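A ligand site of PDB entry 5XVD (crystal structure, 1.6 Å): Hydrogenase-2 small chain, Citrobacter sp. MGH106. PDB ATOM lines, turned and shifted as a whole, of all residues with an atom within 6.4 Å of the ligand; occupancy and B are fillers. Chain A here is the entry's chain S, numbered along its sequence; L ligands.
An iron atom (FE3) of the ligand is bound by a ring nitrogen (ND1) of His 192 (2.2 Å).
N of Arg 198 lies close to S4 of the ligand (3.5 Å).
The side-chain sulfur of Cys 220 is bound to an iron atom (FE1) of the ligand (2.4 Å).
An iron atom (FE2) of the ligand is bound by the side-chain sulfur (SG) of Cys 195.
FE4 of the ligand is bound by SG of Cys 226 (2.4 Å).
The backbone NH of Leu 221 sits close to a sulfur (S3) of the ligand (3.6 Å).
Merely in contact with the ligand: Arg 197 (3.7 Å), Tyr 222 (3.8 Å), Gly 228 (3.9 Å), Val 249 (3.9 Å) and Pro 229 (3.9 Å).
Along chain A the residues within 4 Å of the ligand span positions 192 to 249.
The nearest printed residue that does not touch the ligand is Phe 201 (4.1 Å).
The guanidinium group (NH1) of Arg 198 lies within salt-bridge range of the side-chain carboxylate (OE2) of Glu 193, at 3.1 Å.
The backbone NH (N) of Cys 226 is in hydrogen-bond range of the backbone carbonyl oxygen (O) of Leu 221.
The side-chain sulfur (SG) of Cys 220 sits close to the backbone NH (N) of Tyr 222, at 3.4 Å.
O of Gly 228 lies within hydrogen-bond range of N of His 192.
The backbone carbonyl oxygen (O) of His 192 lies within hydrogen-bond range of the guanidinium group (NH1) of Arg 198, 3.4 Å away.
The side-chain sulfur (SG) of Cys 226 sits close to the backbone NH (N) of Gly 228, 3.4 Å away.
The guanidinium group (NH1) of Arg 197 lies within hydrogen-bond range of the backbone carbonyl oxygen (O) of Trp 219, at 2.9 Å.
The guanidinium group of Arg 197 is in hydrogen-bond range of the backbone carbonyl oxygen of Val 249.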
ATOM      1  N   ILE A 191      -8.092   3.177  28.456  1.00  0.00           N
ATOM      2  CA  ILE A 191      -8.103   2.217  29.571  1.00  0.00           C
ATOM      3  C   ILE A 191      -7.157   1.048  29.299  1.00  0.00           C
ATOM      4  O   ILE A 191      -6.425   0.607  30.186  1.00  0.00           O
ATOM      5  CB  ILE A 191      -9.554   1.734  29.859  1.00  0.00           C
ATOM      6  CG1 ILE A 191     -10.363   2.894  30.478  1.00  0.00           C
ATOM      7  CG2 ILE A 191      -9.580   0.516  30.783  1.00  0.00           C
ATOM      8  CD1 ILE A 191     -11.861   2.694  30.460  1.00  0.00           C
ATOM      9  N   HIS A 192      -7.135   0.589  28.050  1.00  0.00           N
ATOM     10  CA  HIS A 192      -6.295  -0.532  27.610  1.00  0.00           C
ATOM     11  C   HIS A 192      -4.801  -0.195  27.708  1.00  0.00           C
ATOM     12  O   HIS A 192      -3.960  -1.099  27.804  1.00  0.00           O
ATOM     13  CB  HIS A 192      -6.678  -0.890  26.172  1.00  0.00           C
ATOM     14  CG  HIS A 192      -5.898  -2.018  25.558  1.00  0.00           C
ATOM     15  ND1 HIS A 192      -6.078  -3.335  25.915  1.00  0.00           N
ATOM     16  CD2 HIS A 192      -4.976  -2.032  24.565  1.00  0.00           C
ATOM     17  CE1 HIS A 192      -5.296  -4.109  25.201  1.00  0.00           C
ATOM     18  NE2 HIS A 192      -4.613  -3.345  24.370  1.00  0.00           N
ATOM     19  N   GLU A 193      -4.486   1.099  27.692  1.00  0.00           N
ATOM     20  CA  GLU A 193      -3.095   1.543  27.777  1.00  0.00           C
ATOM     21  C   GLU A 193      -2.658   1.786  29.221  1.00  0.00           C
ATOM     22  O   GLU A 193      -1.576   2.323  29.469  1.00  0.00           O
ATOM     23  CB  GLU A 193      -2.879   2.770  26.899  1.00  0.00           C
ATOM     24  CG  GLU A 193      -3.051   2.460  25.406  1.00  0.00           C
ATOM     25  CD  GLU A 193      -2.065   1.405  24.921  1.00  0.00           C
ATOM     26  OE1 GLU A 193      -0.848   1.573  25.140  1.00  0.00           O
ATOM     27  OE2 GLU A 193      -2.500   0.398  24.316  1.00  0.00           O
ATOM     28  N   CYS A 195      -4.075  -0.838  31.723  1.00  0.00           N
ATOM     29  CA  CYS A 195      -4.850  -1.928  32.305  1.00  0.00           C
ATOM     30  C   CYS A 195      -3.976  -3.069  32.825  1.00  0.00           C
ATOM     31  O   CYS A 195      -3.079  -3.558  32.120  1.00  0.00           O
ATOM     32  CB  CYS A 195      -5.836  -2.490  31.286  1.00  0.00           C
ATOM     33  SG  CYS A 195      -6.821  -3.846  31.967  1.00  0.00           S
ATOM     34  N   GLU A 196      -4.261  -3.491  34.041  1.00  0.00           N
ATOM     35  CA  GLU A 196      -3.465  -4.544  34.686  1.00  0.00           C
ATOM     36  C   GLU A 196      -3.618  -5.916  34.044  1.00  0.00           C
ATOM     37  O   GLU A 196      -2.855  -6.824  34.359  1.00  0.00           O
ATOM     38  CB  GLU A 196      -3.791  -4.600  36.178  1.00  0.00           C
ATOM     39  CG  GLU A 196      -5.184  -5.122  36.491  1.00  0.00           C
ATOM     40  CD  GLU A 196      -6.269  -4.055  36.558  1.00  0.00           C
ATOM     41  OE1 GLU A 196      -6.096  -2.955  35.964  1.00  0.00           O
ATOM     42  OE2 GLU A 196      -7.291  -4.341  37.219  1.00  0.00           O
ATOM     43  N   ARG A 197      -4.603  -6.097  33.160  1.00  0.00           N
ATOM     44  CA  ARG A 197      -4.724  -7.375  32.452  1.00  0.00           C
ATOM     45  C   ARG A 197      -3.999  -7.405  31.111  1.00  0.00           C
ATOM     46  O   ARG A 197      -4.034  -8.405  30.413  1.00  0.00           O
ATOM     47  CB  ARG A 197      -6.178  -7.808  32.280  1.00  0.00           C
ATOM     48  CG  ARG A 197      -6.892  -7.831  33.632  1.00  0.00           C
ATOM     49  CD  ARG A 197      -8.181  -8.625  33.630  1.00  0.00           C
ATOM     50  NE  ARG A 197      -8.712  -8.697  34.985  1.00  0.00           N
ATOM     51  CZ  ARG A 197      -9.647  -9.543  35.382  1.00  0.00           C
ATOM     52  NH1 ARG A 197     -10.167 -10.412  34.516  1.00  0.00           N
ATOM     53  NH2 ARG A 197     -10.057  -9.535  36.645  1.00  0.00           N
ATOM     54  N   ARG A 198      -3.349  -6.295  30.773  1.00  0.00           N
ATOM     55  CA  ARG A 198      -2.567  -6.237  29.545  1.00  0.00           C
ATOM     56  C   ARG A 198      -1.541  -7.373  29.378  1.00  0.00           C
ATOM     57  O   ARG A 198      -1.379  -7.886  28.265  1.00  0.00           O
ATOM     58  CB  ARG A 198      -1.885  -4.863  29.414  1.00  0.00           C
ATOM     59  CG  ARG A 198      -1.093  -4.714  28.149  1.00  0.00           C
ATOM     60  CD  ARG A 198      -1.943  -4.800  26.869  1.00  0.00           C
ATOM     61  NE  ARG A 198      -1.082  -4.509  25.727  1.00  0.00           N
ATOM     62  CZ  ARG A 198      -0.951  -3.295  25.182  1.00  0.00           C
ATOM     63  NH1 ARG A 198      -1.679  -2.285  25.640  1.00  0.00           N
ATOM     64  NH2 ARG A 198      -0.119  -3.116  24.168  1.00  0.00           N
ATOM     65  N   PRO A 199      -0.857  -7.806  30.465  1.00  0.00           N
ATOM     66  CA  PRO A 199       0.054  -8.952  30.275  1.00  0.00           C
ATOM     67  C   PRO A 199      -0.657 -10.195  29.733  1.00  0.00           C
ATOM     68  O   PRO A 199      -0.068 -10.967  28.965  1.00  0.00           O
ATOM     69  CB  PRO A 199       0.565  -9.222  31.698  1.00  0.00           C
ATOM     70  CG  PRO A 199       0.439  -7.913  32.411  1.00  0.00           C
ATOM     71  CD  PRO A 199      -0.799  -7.270  31.843  1.00  0.00           C
ATOM     72  N   PHE A 201      -3.483 -10.158  27.814  1.00  0.00           N
ATOM     73  CA  PHE A 201      -3.739  -9.803  26.422  1.00  0.00           C
ATOM     74  C   PHE A 201      -2.498 -10.122  25.574  1.00  0.00           C
ATOM     75  O   PHE A 201      -2.594 -10.739  24.516  1.00  0.00           O
ATOM     76  CB  PHE A 201      -4.097  -8.316  26.338  1.00  0.00           C
ATOM     77  CG  PHE A 201      -4.280  -7.812  24.941  1.00  0.00           C
ATOM     78  CD1 PHE A 201      -3.206  -7.300  24.219  1.00  0.00           C
ATOM     79  CD2 PHE A 201      -5.531  -7.818  24.330  1.00  0.00           C
ATOM     80  CE1 PHE A 201      -3.370  -6.831  22.940  1.00  0.00           C
ATOM     81  CE2 PHE A 201      -5.698  -7.337  23.043  1.00  0.00           C
ATOM     82  CZ  PHE A 201      -4.614  -6.846  22.350  1.00  0.00           C
ATOM     83  N   PHE A 206      -6.900 -15.393  27.361  1.00  0.00           N
ATOM     84  CA  PHE A 206      -8.196 -14.725  27.255  1.00  0.00           C
ATOM     85  C   PHE A 206      -9.292 -15.534  27.919  1.00  0.00           C
ATOM     86  O   PHE A 206      -9.382 -16.751  27.729  1.00  0.00           O
ATOM     87  CB  PHE A 206      -8.582 -14.523  25.780  1.00  0.00           C
ATOM     88  CG  PHE A 206      -7.697 -13.590  25.029  1.00  0.00           C
ATOM     89  CD1 PHE A 206      -7.613 -12.255  25.384  1.00  0.00           C
ATOM     90  CD2 PHE A 206      -6.949 -14.038  23.939  1.00  0.00           C
ATOM     91  CE1 PHE A 206      -6.786 -11.394  24.676  1.00  0.00           C
ATOM     92  CE2 PHE A 206      -6.139 -13.178  23.235  1.00  0.00           C
ATOM     93  CZ  PHE A 206      -6.053 -11.854  23.598  1.00  0.00           C
ATOM     94  N   TRP A 219      -7.912 -13.460  33.689  1.00  0.00           N
ATOM     95  CA  TRP A 219      -7.321 -13.194  32.371  1.00  0.00           C
ATOM     96  C   TRP A 219      -8.018 -12.039  31.661  1.00  0.00           C
ATOM     97  O   TRP A 219      -9.039 -11.516  32.124  1.00  0.00           O
ATOM     98  CB  TRP A 219      -7.343 -14.459  31.512  1.00  0.00           C
ATOM     99  CG  TRP A 219      -6.397 -15.515  31.977  1.00  0.00           C
ATOM    100  CD1 TRP A 219      -5.599 -15.478  33.086  1.00  0.00           C
ATOM    101  CD2 TRP A 219      -6.152 -16.775  31.341  1.00  0.00           C
ATOM    102  NE1 TRP A 219      -4.872 -16.652  33.179  1.00  0.00           N
ATOM    103  CE2 TRP A 219      -5.193 -17.461  32.118  1.00  0.00           C
ATOM    104  CE3 TRP A 219      -6.653 -17.396  30.184  1.00  0.00           C
ATOM    105  CZ2 TRP A 219      -4.720 -18.730  31.772  1.00  0.00           C
ATOM    106  CZ3 TRP A 219      -6.187 -18.656  29.853  1.00  0.00           C
ATOM    107  CH2 TRP A 219      -5.229 -19.311  30.649  1.00  0.00           C
ATOM    108  N   CYS A 220      -7.461 -11.636  30.522  1.00  0.00           N
ATOM    109  CA  CYS A 220      -7.954 -10.485  29.772  1.00  0.00           C
ATOM    110  C   CYS A 220      -9.352 -10.756  29.227  1.00  0.00           C
ATOM    111  O   CYS A 220      -9.677 -11.890  28.852  1.00  0.00           O
ATOM    112  CB  CYS A 220      -6.969 -10.157  28.640  1.00  0.00           C
ATOM    113  SG  CYS A 220      -7.597  -9.055  27.365  1.00  0.00           S
ATOM    114  N   LEU A 221     -10.165  -9.704  29.154  1.00  0.00           N
ATOM    115  CA  LEU A 221     -11.588  -9.827  28.798  1.00  0.00           C
ATOM    116  C   LEU A 221     -11.902  -9.352  27.369  1.00  0.00           C
ATOM    117  O   LEU A 221     -13.068  -9.177  27.029  1.00  0.00           O
ATOM    118  CB  LEU A 221     -12.465  -9.059  29.810  1.00  0.00           C
ATOM    119  CG  LEU A 221     -12.251  -9.449  31.280  1.00  0.00           C
ATOM    120  CD1 LEU A 221     -13.207  -8.670  32.210  1.00  0.00           C
ATOM    121  CD2 LEU A 221     -12.363 -10.964  31.524  1.00  0.00           C
ATOM    122  N   TYR A 222     -10.868  -9.169  26.562  1.00  0.00           N
ATOM    123  CA  TYR A 222     -11.021  -8.690  25.181  1.00  0.00           C
ATOM    124  C   TYR A 222     -12.083  -9.468  24.407  1.00  0.00           C
ATOM    125  O   TYR A 222     -12.976  -8.885  23.774  1.00  0.00           O
ATOM    126  CB  TYR A 222      -9.691  -8.773  24.409  1.00  0.00           C
ATOM    127  CG  TYR A 222      -9.736  -8.156  23.021  1.00  0.00           C
ATOM    128  CD1 TYR A 222     -10.178  -8.872  21.910  1.00  0.00           C
ATOM    129  CD2 TYR A 222      -9.334  -6.840  22.820  1.00  0.00           C
ATOM    130  CE1 TYR A 222     -10.215  -8.282  20.643  1.00  0.00           C
ATOM    131  CE2 TYR A 222      -9.359  -6.252  21.572  1.00  0.00           C
ATOM    132  CZ  TYR A 222      -9.805  -6.969  20.485  1.00  0.00           C
ATOM    133  OH  TYR A 222      -9.831  -6.381  19.237  1.00  0.00           O
ATOM    134  N   HIS A 223     -11.995 -10.791  24.454  1.00  0.00           N
ATOM    135  CA  HIS A 223     -12.910 -11.621  23.680  1.00  0.00           C
ATOM    136  C   HIS A 223     -14.287 -11.785  24.313  1.00  0.00           C
ATOM    137  O   HIS A 223     -15.160 -12.452  23.751  1.00  0.00           O
ATOM    138  CB  HIS A 223     -12.264 -12.939  23.318  1.00  0.00           C
ATOM    139  CG  HIS A 223     -11.218 -12.791  22.273  1.00  0.00           C
ATOM    140  ND1 HIS A 223     -11.514 -12.688  20.926  1.00  0.00           N
ATOM    141  CD2 HIS A 223      -9.869 -12.632  22.372  1.00  0.00           C
ATOM    142  CE1 HIS A 223     -10.398 -12.526  20.246  1.00  0.00           C
ATOM    143  NE2 HIS A 223      -9.385 -12.485  21.088  1.00  0.00           N
ATOM    144  N   CYS A 226     -14.525  -6.505  25.638  1.00  0.00           N
ATOM    145  CA  CYS A 226     -13.974  -5.350  26.359  1.00  0.00           C
ATOM    146  C   CYS A 226     -13.696  -4.161  25.446  1.00  0.00           C
ATOM    147  O   CYS A 226     -13.003  -4.287  24.425  1.00  0.00           O
ATOM    148  CB  CYS A 226     -12.697  -5.744  27.098  1.00  0.00           C
ATOM    149  SG  CYS A 226     -12.127  -4.428  28.209  1.00  0.00           S
ATOM    150  N   LYS A 227     -14.231  -3.003  25.818  1.00  0.00           N
ATOM    151  CA  LYS A 227     -14.036  -1.796  25.031  1.00  0.00           C
ATOM    152  C   LYS A 227     -12.903  -0.923  25.554  1.00  0.00           C
ATOM    153  O   LYS A 227     -12.729   0.203  25.082  1.00  0.00           O
ATOM    154  CB  LYS A 227     -15.331  -0.991  24.981  1.00  0.00           C
ATOM    155  CG  LYS A 227     -16.543  -1.790  24.539  1.00  0.00           C
ATOM    156  CD  LYS A 227     -16.314  -2.446  23.179  1.00  0.00           C
ATOM    157  CE  LYS A 227     -17.610  -3.005  22.604  1.00  0.00           C
ATOM    158  NZ  LYS A 227     -18.288  -3.971  23.535  1.00  0.00           N
ATOM    159  N   GLY A 228     -12.126  -1.432  26.504  1.00  0.00           N
ATOM    160  CA  GLY A 228     -10.939  -0.725  26.951  1.00  0.00           C
ATOM    161  C   GLY A 228     -10.026  -0.214  25.838  1.00  0.00           C
ATOM    162  O   GLY A 228      -9.487   0.886  25.945  1.00  0.00           O
ATOM    163  N   PRO A 229      -9.812  -1.011  24.770  1.00  0.00           N
ATOM    164  CA  PRO A 229      -8.967  -0.552  23.670  1.00  0.00           C
ATOM    165  C   PRO A 229      -9.444   0.699  22.918  1.00  0.00           C
ATOM    166  O   PRO A 229      -8.656   1.293  22.174  1.00  0.00           O
ATOM    167  CB  PRO A 229      -8.945  -1.762  22.723  1.00  0.00           C
ATOM    168  CG  PRO A 229      -9.044  -2.922  23.653  1.00  0.00           C
ATOM    169  CD  PRO A 229     -10.017  -2.479  24.716  1.00  0.00           C
ATOM    170  N   TRP A 247     -13.326  -2.032  39.835  1.00  0.00           N
ATOM    171  CA  TRP A 247     -13.769  -1.477  38.562  1.00  0.00           C
ATOM    172  C   TRP A 247     -14.348  -2.638  37.768  1.00  0.00           C
ATOM    173  O   TRP A 247     -14.177  -3.781  38.160  1.00  0.00           O
ATOM    174  CB  TRP A 247     -12.681  -0.685  37.828  1.00  0.00           C
ATOM    175  CG  TRP A 247     -11.513  -1.424  37.238  1.00  0.00           C
ATOM    176  CD1 TRP A 247     -10.524  -2.073  37.919  1.00  0.00           C
ATOM    177  CD2 TRP A 247     -11.175  -1.512  35.851  1.00  0.00           C
ATOM    178  NE1 TRP A 247      -9.603  -2.598  37.032  1.00  0.00           N
ATOM    179  CE2 TRP A 247      -9.980  -2.241  35.757  1.00  0.00           C
ATOM    180  CE3 TRP A 247     -11.768  -1.042  34.671  1.00  0.00           C
ATOM    181  CZ2 TRP A 247      -9.357  -2.523  34.533  1.00  0.00           C
ATOM    182  CZ3 TRP A 247     -11.156  -1.316  33.450  1.00  0.00           C
ATOM    183  CH2 TRP A 247      -9.967  -2.054  33.397  1.00  0.00           C
ATOM    184  N   VAL A 249     -13.735  -4.367  35.020  1.00  0.00           N
ATOM    185  CA  VAL A 249     -12.859  -5.449  34.586  1.00  0.00           C
ATOM    186  C   VAL A 249     -12.322  -6.259  35.769  1.00  0.00           C
ATOM    187  O   VAL A 249     -12.271  -7.480  35.723  1.00  0.00           O
ATOM    188  CB  VAL A 249     -11.714  -4.915  33.683  1.00  0.00           C
ATOM    189  CG1 VAL A 249     -10.589  -5.936  33.531  1.00  0.00           C
ATOM    190  CG2 VAL A 249     -12.268  -4.500  32.329  1.00  0.00           C
ATOM    191  N   PRO A 254     -16.311  -7.148  31.078  1.00  0.00           N
ATOM    192  CA  PRO A 254     -15.630  -6.231  30.153  1.00  0.00           C
ATOM    193  C   PRO A 254     -16.073  -4.776  30.301  1.00  0.00           C
ATOM    194  O   PRO A 254     -17.213  -4.508  30.686  1.00  0.00           O
ATOM    195  CB  PRO A 254     -16.035  -6.753  28.766  1.00  0.00           C
ATOM    196  CG  PRO A 254     -17.281  -7.571  29.000  1.00  0.00           C
ATOM    197  CD  PRO A 254     -17.053  -8.200  30.356  1.00  0.00           C
ATOM    198  N   CYS A 255     -15.176  -3.852  30.002  1.00  0.00           N
ATOM    199  CA  CYS A 255     -15.566  -2.460  29.823  1.00  0.00           C
ATOM    200  C   CYS A 255     -16.575  -2.391  28.689  1.00  0.00           C
ATOM    201  O   CYS A 255     -16.425  -3.082  27.678  1.00  0.00           O
ATOM    202  CB  CYS A 255     -14.328  -1.615  29.506  1.00  0.00           C
ATOM    203  SG  CYS A 255     -14.665   0.088  29.000  1.00  0.00           S
HETATM  204 FE1  LIG L   1      -7.834  -6.848  28.214  1.00  0.00          FE
HETATM  205 FE2  LIG L   1      -7.646  -4.795  29.961  1.00  0.00          FE
HETATM  206 FE3  LIG L   1      -7.384  -4.340  27.354  1.00  0.00          FE
HETATM  207 FE4  LIG L   1      -9.817  -4.917  28.408  1.00  0.00          FE
HETATM  208  S1  LIG L   1      -8.573  -3.152  28.785  1.00  0.00           S
HETATM  209  S2  LIG L   1      -8.872  -5.754  26.587  1.00  0.00           S
HETATM  210  S3  LIG L   1      -9.144  -6.380  29.934  1.00  0.00           S
HETATM  211  S4  LIG L   1      -6.079  -5.610  28.633  1.00  0.00           S
